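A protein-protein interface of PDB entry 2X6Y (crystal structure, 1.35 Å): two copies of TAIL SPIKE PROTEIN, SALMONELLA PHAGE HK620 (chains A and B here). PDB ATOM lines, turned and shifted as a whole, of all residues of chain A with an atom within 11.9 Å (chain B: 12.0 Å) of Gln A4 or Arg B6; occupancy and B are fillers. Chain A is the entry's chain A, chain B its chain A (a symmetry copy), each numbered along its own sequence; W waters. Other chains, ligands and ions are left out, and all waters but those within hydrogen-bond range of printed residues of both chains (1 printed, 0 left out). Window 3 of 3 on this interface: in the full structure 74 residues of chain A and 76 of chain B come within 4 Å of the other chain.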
ATOM      1  N   GLN A   4      -5.453  -1.271   1.731  1.00  0.00           N
ATOM      2  CA  GLN A   4      -5.291  -1.075   0.248  1.00  0.00           C
ATOM      3  C   GLN A   4      -4.320   0.079  -0.084  1.00  0.00           C
ATOM      4  O   GLN A   4      -3.380  -0.063  -0.877  1.00  0.00           O
ATOM      5  CB  GLN A   4      -6.676  -0.862  -0.420  1.00  0.00           C
ATOM      6  CG  GLN A   4      -7.415   0.502  -0.200  1.00  0.00           C
ATOM      7  CD  GLN A   4      -7.975   0.730   1.235  1.00  0.00           C
ATOM      8  OE1 GLN A   4      -7.239   1.077   2.169  1.00  0.00           O
ATOM      9  NE2 GLN A   4      -9.286   0.575   1.385  1.00  0.00           N
ATOM     10  N   PHE A   5      -4.557   1.221   0.546  1.00  0.00           N
ATOM     11  CA  PHE A   5      -3.674   2.363   0.415  1.00  0.00           C
ATOM     12  C   PHE A   5      -2.353   2.027   1.121  1.00  0.00           C
ATOM     13  O   PHE A   5      -1.266   2.324   0.612  1.00  0.00           O
ATOM     14  CB  PHE A   5      -4.318   3.581   1.064  1.00  0.00           C
ATOM     15  CG  PHE A   5      -3.505   4.828   0.936  1.00  0.00           C
ATOM     16  CD1 PHE A   5      -3.097   5.276  -0.318  1.00  0.00           C
ATOM     17  CD2 PHE A   5      -3.147   5.553   2.056  1.00  0.00           C
ATOM     18  CE1 PHE A   5      -2.355   6.428  -0.441  1.00  0.00           C
ATOM     19  CE2 PHE A   5      -2.415   6.718   1.939  1.00  0.00           C
ATOM     20  CZ  PHE A   5      -2.010   7.149   0.690  1.00  0.00           C
ATOM     21  N   ARG A   6      -2.462   1.404   2.292  1.00  0.00           N
ATOM     22  CA  ARG A   6      -1.293   1.074   3.119  1.00  0.00           C
ATOM     23  C   ARG A   6      -0.329   0.172   2.356  1.00  0.00           C
ATOM     24  O   ARG A   6       0.900   0.361   2.416  1.00  0.00           O
ATOM     25  CB  ARG A   6      -1.732   0.386   4.419  1.00  0.00           C
ATOM     26  CG  ARG A   6      -0.554  -0.036   5.335  1.00  0.00           C
ATOM     27  CD  ARG A   6      -0.786  -1.364   6.055  1.00  0.00           C
ATOM     28  NE  ARG A   6      -1.001  -1.227   7.494  1.00  0.00           N
ATOM     29  CZ  ARG A   6      -0.047  -1.268   8.427  1.00  0.00           C
ATOM     30  NH1 ARG A   6       1.238  -1.411   8.098  1.00  0.00           N
ATOM     31  NH2 ARG A   6      -0.378  -1.144   9.715  1.00  0.00           N
ATOM     32  N   ALA A   7      -0.883  -0.811   1.650  1.00  0.00           N
ATOM     33  CA  ALA A   7      -0.094  -1.696   0.809  1.00  0.00           C
ATOM     34  C   ALA A   7       0.677  -0.920  -0.267  1.00  0.00           C
ATOM     35  O   ALA A   7       1.862  -1.172  -0.470  1.00  0.00           O
ATOM     36  CB  ALA A   7      -0.994  -2.754   0.165  1.00  0.00           C
ATOM     37  N   ILE A   8       0.004   0.020  -0.936  1.00  0.00           N
ATOM     38  CA  ILE A   8       0.638   0.852  -1.978  1.00  0.00           C
ATOM     39  C   ILE A   8       1.800   1.633  -1.349  1.00  0.00           C
ATOM     40  O   ILE A   8       2.911   1.647  -1.882  1.00  0.00           O
ATOM     41  CB  ILE A   8      -0.387   1.827  -2.660  1.00  0.00           C
ATOM     42  CG1 ILE A   8      -1.354   1.047  -3.576  1.00  0.00           C
ATOM     43  CG2 ILE A   8       0.317   2.927  -3.435  1.00  0.00           C
ATOM     44  CD1 ILE A   8      -2.628   1.847  -4.040  1.00  0.00           C
ATOM     45  N   ILE A   9       1.545   2.254  -0.203  1.00  0.00           N
ATOM     46  CA  ILE A   9       2.534   3.140   0.423  1.00  0.00           C
ATOM     47  C   ILE A   9       3.792   2.379   0.830  1.00  0.00           C
ATOM     48  O   ILE A   9       4.895   2.904   0.701  1.00  0.00           O
ATOM     49  CB  ILE A   9       1.922   3.913   1.616  1.00  0.00           C
ATOM     50  CG1 ILE A   9       0.893   4.933   1.113  1.00  0.00           C
ATOM     51  CG2 ILE A   9       3.016   4.639   2.459  1.00  0.00           C
ATOM     52  CD1 ILE A   9       1.496   6.086   0.299  1.00  0.00           C
ATOM     53  N   GLU A  10       3.627   1.146   1.310  1.00  0.00           N
ATOM     54  CA  GLU A  10       4.758   0.334   1.753  1.00  0.00           C
ATOM     55  C   GLU A  10       5.482  -0.389   0.608  1.00  0.00           C
ATOM     56  O   GLU A  10       6.593  -0.882   0.787  1.00  0.00           O
ATOM     57  CB  GLU A  10       4.307  -0.659   2.839  1.00  0.00           C
ATOM     58  CG  GLU A  10       3.893   0.031   4.127  1.00  0.00           C
ATOM     59  CD  GLU A  10       3.817  -0.904   5.321  1.00  0.00           C
ATOM     60  OE1 GLU A  10       2.810  -1.640   5.441  1.00  0.00           O
ATOM     61  OE2 GLU A  10       4.756  -0.881   6.160  1.00  0.00           O
ATOM     62  N   SER A  11       4.845  -0.425  -0.560  1.00  0.00           N
ATOM     63  CA  SER A  11       5.428  -1.045  -1.741  1.00  0.00           C
ATOM     64  C   SER A  11       6.479  -0.130  -2.363  1.00  0.00           C
ATOM     65  O   SER A  11       6.545   1.045  -2.015  1.00  0.00           O
ATOM     66  CB  SER A  11       4.339  -1.359  -2.773  1.00  0.00           C
ATOM     67  OG  SER A  11       4.006  -0.239  -3.572  1.00  0.00           O
ATOM     68  N   PRO A  12       7.264  -0.647  -3.329  1.00  0.00           N
ATOM     69  CA  PRO A  12       8.252   0.190  -4.018  1.00  0.00           C
ATOM     70  C   PRO A  12       7.667   1.372  -4.822  1.00  0.00           C
ATOM     71  O   PRO A  12       8.410   2.283  -5.187  1.00  0.00           O
ATOM     72  CB  PRO A  12       8.965  -0.800  -4.955  1.00  0.00           C
ATOM     73  CG  PRO A  12       8.652  -2.124  -4.446  1.00  0.00           C
ATOM     74  CD  PRO A  12       7.333  -2.045  -3.790  1.00  0.00           C
ATOM     75  N   GLU A  13       6.360   1.367  -5.090  1.00  0.00           N
ATOM     76  CA  GLU A  13       5.689   2.519  -5.717  1.00  0.00           C
ATOM     77  C   GLU A  13       5.101   3.535  -4.711  1.00  0.00           C
ATOM     78  O   GLU A  13       4.446   4.511  -5.107  1.00  0.00           O
ATOM     79  CB  GLU A  13       4.576   2.037  -6.653  1.00  0.00           C
ATOM     80  CG  GLU A  13       5.085   1.151  -7.796  1.00  0.00           C
ATOM     81  CD  GLU A  13       4.007   0.761  -8.786  1.00  0.00           C
ATOM     82  OE1 GLU A  13       2.823   1.098  -8.570  1.00  0.00           O
ATOM     83  OE2 GLU A  13       4.355   0.111  -9.796  1.00  0.00           O
ATOM     84  N   GLY A  14       5.339   3.309  -3.417  1.00  0.00           N
ATOM     85  CA  GLY A  14       4.811   4.177  -2.368  1.00  0.00           C
ATOM     86  C   GLY A  14       5.133   5.648  -2.551  1.00  0.00           C
ATOM     87  O   GLY A  14       4.240   6.498  -2.488  1.00  0.00           O
ATOM     88  N   ALA A  15       6.406   5.952  -2.797  1.00  0.00           N
ATOM     89  CA  ALA A  15       6.838   7.344  -2.950  1.00  0.00           C
ATOM     90  C   ALA A  15       6.176   7.991  -4.160  1.00  0.00           C
ATOM     91  O   ALA A  15       6.027   9.209  -4.201  1.00  0.00           O
ATOM     92  CB  ALA A  15       8.359   7.433  -3.065  1.00  0.00           C
ATOM     93  N   GLY A  16       5.789   7.173  -5.140  1.00  0.00           N
ATOM     94  CA  GLY A  16       5.047   7.645  -6.308  1.00  0.00           C
ATOM     95  C   GLY A  16       3.586   7.977  -6.047  1.00  0.00           C
ATOM     96  O   GLY A  16       2.863   8.330  -6.980  1.00  0.00           O
ATOM     97  N   HIS A  17       3.146   7.828  -4.795  1.00  0.00           N
ATOM     98  CA  HIS A  17       1.791   8.170  -4.387  1.00  0.00           C
ATOM     99  C   HIS A  17       1.727   9.287  -3.340  1.00  0.00           C
ATOM    100  O   HIS A  17       0.631   9.739  -2.993  1.00  0.00           O
ATOM    101  CB  HIS A  17       1.078   6.914  -3.865  1.00  0.00           C
ATOM    102  CG  HIS A  17       0.735   5.934  -4.942  1.00  0.00           C
ATOM    103  ND1 HIS A  17       1.668   5.093  -5.501  1.00  0.00           N
ATOM    104  CD2 HIS A  17      -0.432   5.686  -5.582  1.00  0.00           C
ATOM    105  CE1 HIS A  17       1.087   4.349  -6.428  1.00  0.00           C
ATOM    106  NE2 HIS A  17      -0.187   4.697  -6.504  1.00  0.00           N
ATOM    107  N   VAL A  18       2.881   9.721  -2.825  1.00  0.00           N
ATOM    108  CA  VAL A  18       2.940  10.804  -1.841  1.00  0.00           C
ATOM    109  C   VAL A  18       3.205  12.124  -2.548  1.00  0.00           C
ATOM    110  O   VAL A  18       4.244  12.308  -3.181  1.00  0.00           O
ATOM    111  CB  VAL A  18       4.032  10.554  -0.787  1.00  0.00           C
ATOM    112  CG1 VAL A  18       4.067  11.681   0.247  1.00  0.00           C
ATOM    113  CG2 VAL A  18       3.821   9.193  -0.102  1.00  0.00           C
ATOM    114  N   GLY A  19       2.258  13.046  -2.440  1.00  0.00           N
ATOM    115  CA  GLY A  19       2.340  14.280  -3.206  1.00  0.00           C
ATOM    116  C   GLY A  19       3.335  15.268  -2.637  1.00  0.00           C
ATOM    117  O   GLY A  19       3.632  15.245  -1.435  1.00  0.00           O
ATOM    118  N   TYR A  20       3.849  16.125  -3.515  1.00  0.00           N
ATOM    119  CA  TYR A  20       4.822  17.138  -3.141  1.00  0.00           C
ATOM    120  C   TYR A  20       4.716  18.348  -4.050  1.00  0.00           C
ATOM    121  O   TYR A  20       4.522  18.213  -5.271  1.00  0.00           O
ATOM    122  CB  TYR A  20       6.240  16.564  -3.222  1.00  0.00           C
ATOM    123  CG  TYR A  20       7.365  17.570  -3.073  1.00  0.00           C
ATOM    124  CD1 TYR A  20       7.699  18.109  -1.817  1.00  0.00           C
ATOM    125  CD2 TYR A  20       8.098  17.991  -4.189  1.00  0.00           C
ATOM    126  CE1 TYR A  20       8.728  19.035  -1.686  1.00  0.00           C
ATOM    127  CE2 TYR A  20       9.129  18.931  -4.073  1.00  0.00           C
ATOM    128  CZ  TYR A  20       9.438  19.447  -2.829  1.00  0.00           C
ATOM    129  OH  TYR A  20      10.480  20.343  -2.703  1.00  0.00           O
ATOM    130  N   ARG A  31       3.937  17.327  -7.908  1.00  0.00           N
ATOM    131  CA  ARG A  31       4.759  16.147  -8.189  1.00  0.00           C
ATOM    132  C   ARG A  31       4.464  15.087  -7.149  1.00  0.00           C
ATOM    133  O   ARG A  31       3.640  15.297  -6.243  1.00  0.00           O
ATOM    134  CB  ARG A  31       6.259  16.514  -8.145  1.00  0.00           C
ATOM    135  CG  ARG A  31       6.614  17.795  -8.925  1.00  0.00           C
ATOM    136  CD  ARG A  31       8.082  18.134  -8.806  1.00  0.00           C
ATOM    137  NE  ARG A  31       8.922  17.199  -9.557  1.00  0.00           N
ATOM    138  CZ  ARG A  31      10.250  17.183  -9.510  1.00  0.00           C
ATOM    139  NH1 ARG A  31      10.905  18.044  -8.739  1.00  0.00           N
ATOM    140  NH2 ARG A  31      10.920  16.317 -10.248  1.00  0.00           N
ATOM    141  N   MET A  32       5.134  13.950  -7.287  1.00  0.00           N
ATOM    142  CA  MET A  32       5.195  12.927  -6.236  1.00  0.00           C
ATOM    143  C   MET A  32       6.626  12.869  -5.675  1.00  0.00           C
ATOM    144  O   MET A  32       7.595  13.262  -6.336  1.00  0.00           O
ATOM    145  CB  MET A  32       4.767  11.566  -6.793  1.00  0.00           C
ATOM    146  CG  MET A  32       3.332  11.548  -7.279  1.00  0.00           C
ATOM    147  SD  MET A  32       2.176  11.653  -5.891  1.00  0.00           S
ATOM    148  CE  MET A  32       0.845  12.626  -6.585  1.00  0.00           C
ATOM    149  N   GLN B   4      -9.433  10.287   4.924  1.00  0.00           N
ATOM    150  CA  GLN B   4      -9.040  11.659   5.404  1.00  0.00           C
ATOM    151  C   GLN B   4      -7.509  11.858   5.405  1.00  0.00           C
ATOM    152  O   GLN B   4      -6.976  12.841   4.871  1.00  0.00           O
ATOM    153  CB  GLN B   4      -9.652  11.934   6.803  1.00  0.00           C
ATOM    154  CG  GLN B   4      -9.045  11.197   8.047  1.00  0.00           C
ATOM    155  CD  GLN B   4      -9.340   9.670   8.122  1.00  0.00           C
ATOM    156  OE1 GLN B   4      -8.706   8.855   7.438  1.00  0.00           O
ATOM    157  NE2 GLN B   4     -10.273   9.295   8.991  1.00  0.00           N
ATOM    158  N   PHE B   5      -6.811  10.905   6.005  1.00  0.00           N
ATOM    159  CA  PHE B   5      -5.361  10.900   6.001  1.00  0.00           C
ATOM    160  C   PHE B   5      -4.890  10.610   4.569  1.00  0.00           C
ATOM    161  O   PHE B   5      -3.948  11.236   4.069  1.00  0.00           O
ATOM    162  CB  PHE B   5      -4.854   9.822   6.948  1.00  0.00           C
ATOM    163  CG  PHE B   5      -3.365   9.772   7.054  1.00  0.00           C
ATOM    164  CD1 PHE B   5      -2.645  10.911   7.405  1.00  0.00           C
ATOM    165  CD2 PHE B   5      -2.679   8.598   6.805  1.00  0.00           C
ATOM    166  CE1 PHE B   5      -1.274  10.868   7.513  1.00  0.00           C
ATOM    167  CE2 PHE B   5      -1.305   8.543   6.925  1.00  0.00           C
ATOM    168  CZ  PHE B   5      -0.601   9.682   7.268  1.00  0.00           C
ATOM    169  N   ARG B   6      -5.558   9.659   3.919  1.00  0.00           N
ATOM    170  CA  ARG B   6      -5.186   9.221   2.567  1.00  0.00           C
ATOM    171  C   ARG B   6      -5.240  10.388   1.587  1.00  0.00           C
ATOM    172  O   ARG B   6      -4.349  10.539   0.731  1.00  0.00           O
ATOM    173  CB  ARG B   6      -6.116   8.098   2.092  1.00  0.00           C
ATOM    174  CG  ARG B   6      -5.819   7.603   0.652  1.00  0.00           C
ATOM    175  CD  ARG B   6      -7.075   7.242  -0.140  1.00  0.00           C
ATOM    176  NE  ARG B   6      -7.232   5.809  -0.380  1.00  0.00           N
ATOM    177  CZ  ARG B   6      -6.773   5.147  -1.445  1.00  0.00           C
ATOM    178  NH1 ARG B   6      -6.074   5.767  -2.397  1.00  0.00           N
ATOM    179  NH2 ARG B   6      -6.996   3.834  -1.552  1.00  0.00           N
ATOM    180  N   ALA B   7      -6.286  11.204   1.706  1.00  0.00           N
ATOM    181  CA  ALA B   7      -6.425  12.401   0.895  1.00  0.00           C
ATOM    182  C   ALA B   7      -5.244  13.361   1.091  1.00  0.00           C
ATOM    183  O   ALA B   7      -4.704  13.871   0.112  1.00  0.00           O
ATOM    184  CB  ALA B   7      -7.746  13.105   1.217  1.00  0.00           C
ATOM    185  N   ILE B   8      -4.849  13.588   2.347  1.00  0.00           N
ATOM    186  CA  ILE B   8      -3.710  14.472   2.666  1.00  0.00           C
ATOM    187  C   ILE B   8      -2.447  13.913   1.996  1.00  0.00           C
ATOM    188  O   ILE B   8      -1.710  14.643   1.331  1.00  0.00           O
ATOM    189  CB  ILE B   8      -3.500  14.627   4.215  1.00  0.00           C
ATOM    190  CG1 ILE B   8      -4.616  15.496   4.831  1.00  0.00           C
ATOM    191  CG2 ILE B   8      -2.132  15.201   4.538  1.00  0.00           C
ATOM    192  CD1 ILE B   8      -4.716  15.443   6.402  1.00  0.00           C
ATOM    193  N   ILE B   9      -2.219  12.614   2.151  1.00  0.00           N
ATOM    194  CA  ILE B   9      -0.978  11.993   1.673  1.00  0.00           C
ATOM    195  C   ILE B   9      -0.852  12.086   0.156  1.00  0.00           C
ATOM    196  O   ILE B   9       0.244  12.295  -0.357  1.00  0.00           O
ATOM    197  CB  ILE B   9      -0.853  10.533   2.168  1.00  0.00           C
ATOM    198  CG1 ILE B   9      -0.626  10.506   3.686  1.00  0.00           C
ATOM    199  CG2 ILE B   9       0.306   9.773   1.449  1.00  0.00           C
ATOM    200  CD1 ILE B   9       0.727  11.082   4.130  1.00  0.00           C
ATOM    201  N   GLU B  10      -1.969  11.938  -0.557  1.00  0.00           N
ATOM    202  CA  GLU B  10      -1.964  11.984  -2.017  1.00  0.00           C
ATOM    203  C   GLU B  10      -1.988  13.409  -2.588  1.00  0.00           C
ATOM    204  O   GLU B  10      -1.719  13.612  -3.770  1.00  0.00           O
ATOM    205  CB  GLU B  10      -3.123  11.142  -2.580  1.00  0.00           C
ATOM    206  CG  GLU B  10      -2.951   9.657  -2.313  1.00  0.00           C
ATOM    207  CD  GLU B  10      -3.846   8.777  -3.168  1.00  0.00           C
ATOM    208  OE1 GLU B  10      -5.050   8.654  -2.841  1.00  0.00           O
ATOM    209  OE2 GLU B  10      -3.337   8.183  -4.153  1.00  0.00           O
ATOM    210  N   SER B  11      -2.294  14.381  -1.730  1.00  0.00           N
ATOM    211  CA  SER B  11      -2.318  15.781  -2.124  1.00  0.00           C
ATOM    212  C   SER B  11      -0.900  16.337  -2.219  1.00  0.00           C
ATOM    213  O   SER B  11       0.034  15.702  -1.738  1.00  0.00           O
ATOM    214  CB  SER B  11      -3.130  16.606  -1.119  1.00  0.00           C
ATOM    215  OG  SER B  11      -2.374  16.978   0.018  1.00  0.00           O
ATOM    216  N   PRO B  12      -0.739  17.551  -2.782  1.00  0.00           N
ATOM    217  CA  PRO B  12       0.585  18.177  -2.848  1.00  0.00           C
ATOM    218  C   PRO B  12       1.237  18.483  -1.482  1.00  0.00           C
ATOM    219  O   PRO B  12       2.442  18.733  -1.427  1.00  0.00           O
ATOM    220  CB  PRO B  12       0.325  19.478  -3.626  1.00  0.00           C
ATOM    221  CG  PRO B  12      -0.957  19.298  -4.285  1.00  0.00           C
ATOM    222  CD  PRO B  12      -1.758  18.382  -3.450  1.00  0.00           C
ATOM    223  N   GLU B  13       0.464  18.459  -0.394  1.00  0.00           N
ATOM    224  CA  GLU B  13       1.023  18.590   0.962  1.00  0.00           C
ATOM    225  C   GLU B  13       1.374  17.242   1.636  1.00  0.00           C
ATOM    226  O   GLU B  13       1.783  17.208   2.806  1.00  0.00           O
ATOM    227  CB  GLU B  13       0.055  19.364   1.861  1.00  0.00           C
ATOM    228  CG  GLU B  13      -0.227  20.787   1.364  1.00  0.00           C
ATOM    229  CD  GLU B  13      -1.098  21.596   2.305  1.00  0.00           C
ATOM    230  OE1 GLU B  13      -1.570  21.050   3.325  1.00  0.00           O
ATOM    231  OE2 GLU B  13      -1.303  22.795   2.018  1.00  0.00           O
ATOM    232  N   GLY B  14       1.219  16.142   0.898  1.00  0.00           N
ATOM    233  CA  GLY B  14       1.485  14.808   1.431  1.00  0.00           C
ATOM    234  C   GLY B  14       2.858  14.644   2.055  1.00  0.00           C
ATOM    235  O   GLY B  14       2.980  14.163   3.184  1.00  0.00           O
ATOM    236  N   ALA B  15       3.894  15.060   1.328  1.00  0.00           N
ATOM    237  CA  ALA B  15       5.269  14.914   1.814  1.00  0.00           C
ATOM    238  C   ALA B  15       5.490  15.731   3.080  1.00  0.00           C
ATOM    239  O   ALA B  15       6.364  15.404   3.878  1.00  0.00           O
ATOM    240  CB  ALA B  15       6.274  15.318   0.737  1.00  0.00           C
ATOM    241  N   GLY B  16       4.701  16.794   3.253  1.00  0.00           N
ATOM    242  CA  GLY B  16       4.732  17.603   4.471  1.00  0.00           C
ATOM    243  C   GLY B  16       4.082  16.959   5.686  1.00  0.00           C
ATOM    244  O   GLY B  16       4.009  17.584   6.743  1.00  0.00           O
ATOM    245  N   HIS B  17       3.580  15.732   5.523  1.00  0.00           N
ATOM    246  CA  HIS B  17       2.988  14.969   6.613  1.00  0.00           C
ATOM    247  C   HIS B  17       3.733  13.666   6.926  1.00  0.00           C
ATOM    248  O   HIS B  17       3.391  12.986   7.899  1.00  0.00           O
ATOM    249  CB  HIS B  17       1.516  14.673   6.294  1.00  0.00           C
ATOM    250  CG  HIS B  17       0.635  15.879   6.376  1.00  0.00           C
ATOM    251  ND1 HIS B  17       0.591  16.832   5.385  1.00  0.00           N
ATOM    252  CD2 HIS B  17      -0.210  16.300   7.345  1.00  0.00           C
ATOM    253  CE1 HIS B  17      -0.262  17.782   5.730  1.00  0.00           C
ATOM    254  NE2 HIS B  17      -0.754  17.489   6.923  1.00  0.00           N
ATOM    255  N   VAL B  18       4.728  13.308   6.110  1.00  0.00           N
ATOM    256  CA  VAL B  18       5.526  12.101   6.334  1.00  0.00           C
ATOM    257  C   VAL B  18       6.794  12.458   7.092  1.00  0.00           C
ATOM    258  O   VAL B  18       7.629  13.221   6.609  1.00  0.00           O
ATOM    259  CB  VAL B  18       5.893  11.412   5.008  1.00  0.00           C
ATOM    260  CG1 VAL B  18       6.706  10.139   5.257  1.00  0.00           C
ATOM    261  CG2 VAL B  18       4.627  11.098   4.192  1.00  0.00           C
HETATM  262  O   HOH W   1      -1.106   9.717  -5.221  1.00  0.00           O
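CG of Gln A4 touches NH2 of Arg B6, 3.6 Å away.
Arg B6 touches Phe A5 (CG to CG, 3.6 Å).
Ile B9 touches His A17.
CA of Glu B10 touches O of His A17, 3.6 Å away.
O of Ile B9 touches CA of Val A18, at 3.4 Å.
Val A18 touches Gly B14 (CG1 to C, 3.7 Å).
N of Ala B15 touches CG1 of Val A18, 3.6 Å away.
Pro B12 touches Gly A19 (O to O, 3.7 Å).
CA of Tyr A20 touches O of Pro B12 (3.3 Å).
Glu B10 touches Met A32.
Gln A4 touches Arg B6, but with the chains exchanged Arg A6 does not touch Gln B4 (11.0 Å).
Phe A5 touches Arg B6, but with the chains exchanged Arg A6 does not touch Phe B5 (8.4 Å).
His A17 touches Ile B9, but with the chains exchanged Ile A9 does not touch His B17 (10.0 Å).
Val A18 touches Ala B15, but with the chains exchanged Ala A15 does not touch Val B18 (8.4 Å).
Positions printed for both chains: 4, 5, 6, 7, 8, 9, 10, 11, 12, 13, 14, 15, 16, 17 and 18.
Of chain B, only Arg B6 (3.6 Å) comes within 4 Å of Gln A4.
Of chain A, only Gln A4 and Phe A5 come within 4 Å of Arg B6.
Phe A5 touches just these residues of chain B: Arg B6 (3.6 Å), Ile B9 (3.6 Å) and Glu B10 (3.8 Å).
No residue of chain A comes within 4 Å of Gln B4.
No residue of chain A comes within 4 Å of Phe B5.
Ala B7 touches none of the printed residues of chain A.
No residue of chain A comes within 4 Å of Ile B8.
Ile B9 touches just these residues of chain A: Phe A5, His A17, Val A18 and Gly A19.
Of chain A, only Gly A19 (3.1 Å) comes within 4 Å of Ser B11.
Printed residues of chain B within 4 Å of Gly A19: Ile B9 (3.0 Å), Ser B11 (3.1 Å), Pro B12 (3.7 Å), Gly B14 (3.5 Å) and Ala B15 (2.8 Å).
Of the printed residues of chain A, Gly B14 touches Val A18 (3.7 Å) and Gly A19 (3.5 Å).
Printed residues of chain A within 4 Å of Pro B12: Gly A19 and Tyr A20.
Of the printed residues of chain B, Val A18 touches Ile B9 (3.4 Å), Gly B14 (3.7 Å) and Ala B15 (3.6 Å).
Printed residues of chain A within 4 Å of Ala B15: Val A18 and Gly A19.
Arg A31 touches none of the printed residues of chain B.
The nearest residue of chain B that does not touch Gln A4 is Glu B10 (8.9 Å).
The nearest residue of chain A that does not touch Arg B6 is Ile A8 (5.4 Å).
N of Gly A19 is in hydrogen-bond range of O of Ile B9 (3.0 Å).
The backbone NH (N) of Gly B14 lies within hydrogen-bond range of the backbone carbonyl oxygen (O) of Gly A19 (3.5 Å).
The backbone carbonyl oxygen of Gly A19 is in hydrogen-bond range of the backbone NH of Ala B15, 2.8 Å away.
Water W1 lies within hydrogen-bond range of the backbone carbonyl oxygen (O) of His A17 (2.8 Å) and the side-chain carboxylate (OE2) of Glu B10 (2.9 Å).
Hydrophobic or aromatic side chains of chain A that line the printed part of chain B: Phe A5, Val A18 and Met A32.
Of the 15 printed residues of chain B, 7 touch a printed residue of chain A.
Hydrophobic or aromatic side chains of chain B within 4 Å of the printed part of chain A: Ile B9 and Ala B15.
Among the printed residues, no Asp or Glu carboxylate lies within 4 Å of a Lys or Arg side-chain nitrogen of the other chain.
SD of Met A32 lies close to N of Val A18 (3.7 Å).
The backbone NH (N) of Gly A19 lies within hydrogen-bond range of the side-chain sulfur (SD) of Met A32 (3.7 Å).
O of Tyr A20 lies within hydrogen-bond range of N of Arg A31 (2.8 Å).
The backbone carbonyl oxygen of Ile B8 is in hydrogen-bond range of the side-chain hydroxyl of Ser B11, at 2.8 Å.
The backbone NH (N) of Gly B14 lies close to the backbone carbonyl oxygen (O) of Ile B8 (3.3 Å).
The backbone NH of Glu B13 sits close to the side-chain hydroxyl of Ser B11, 3.2 Å away.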
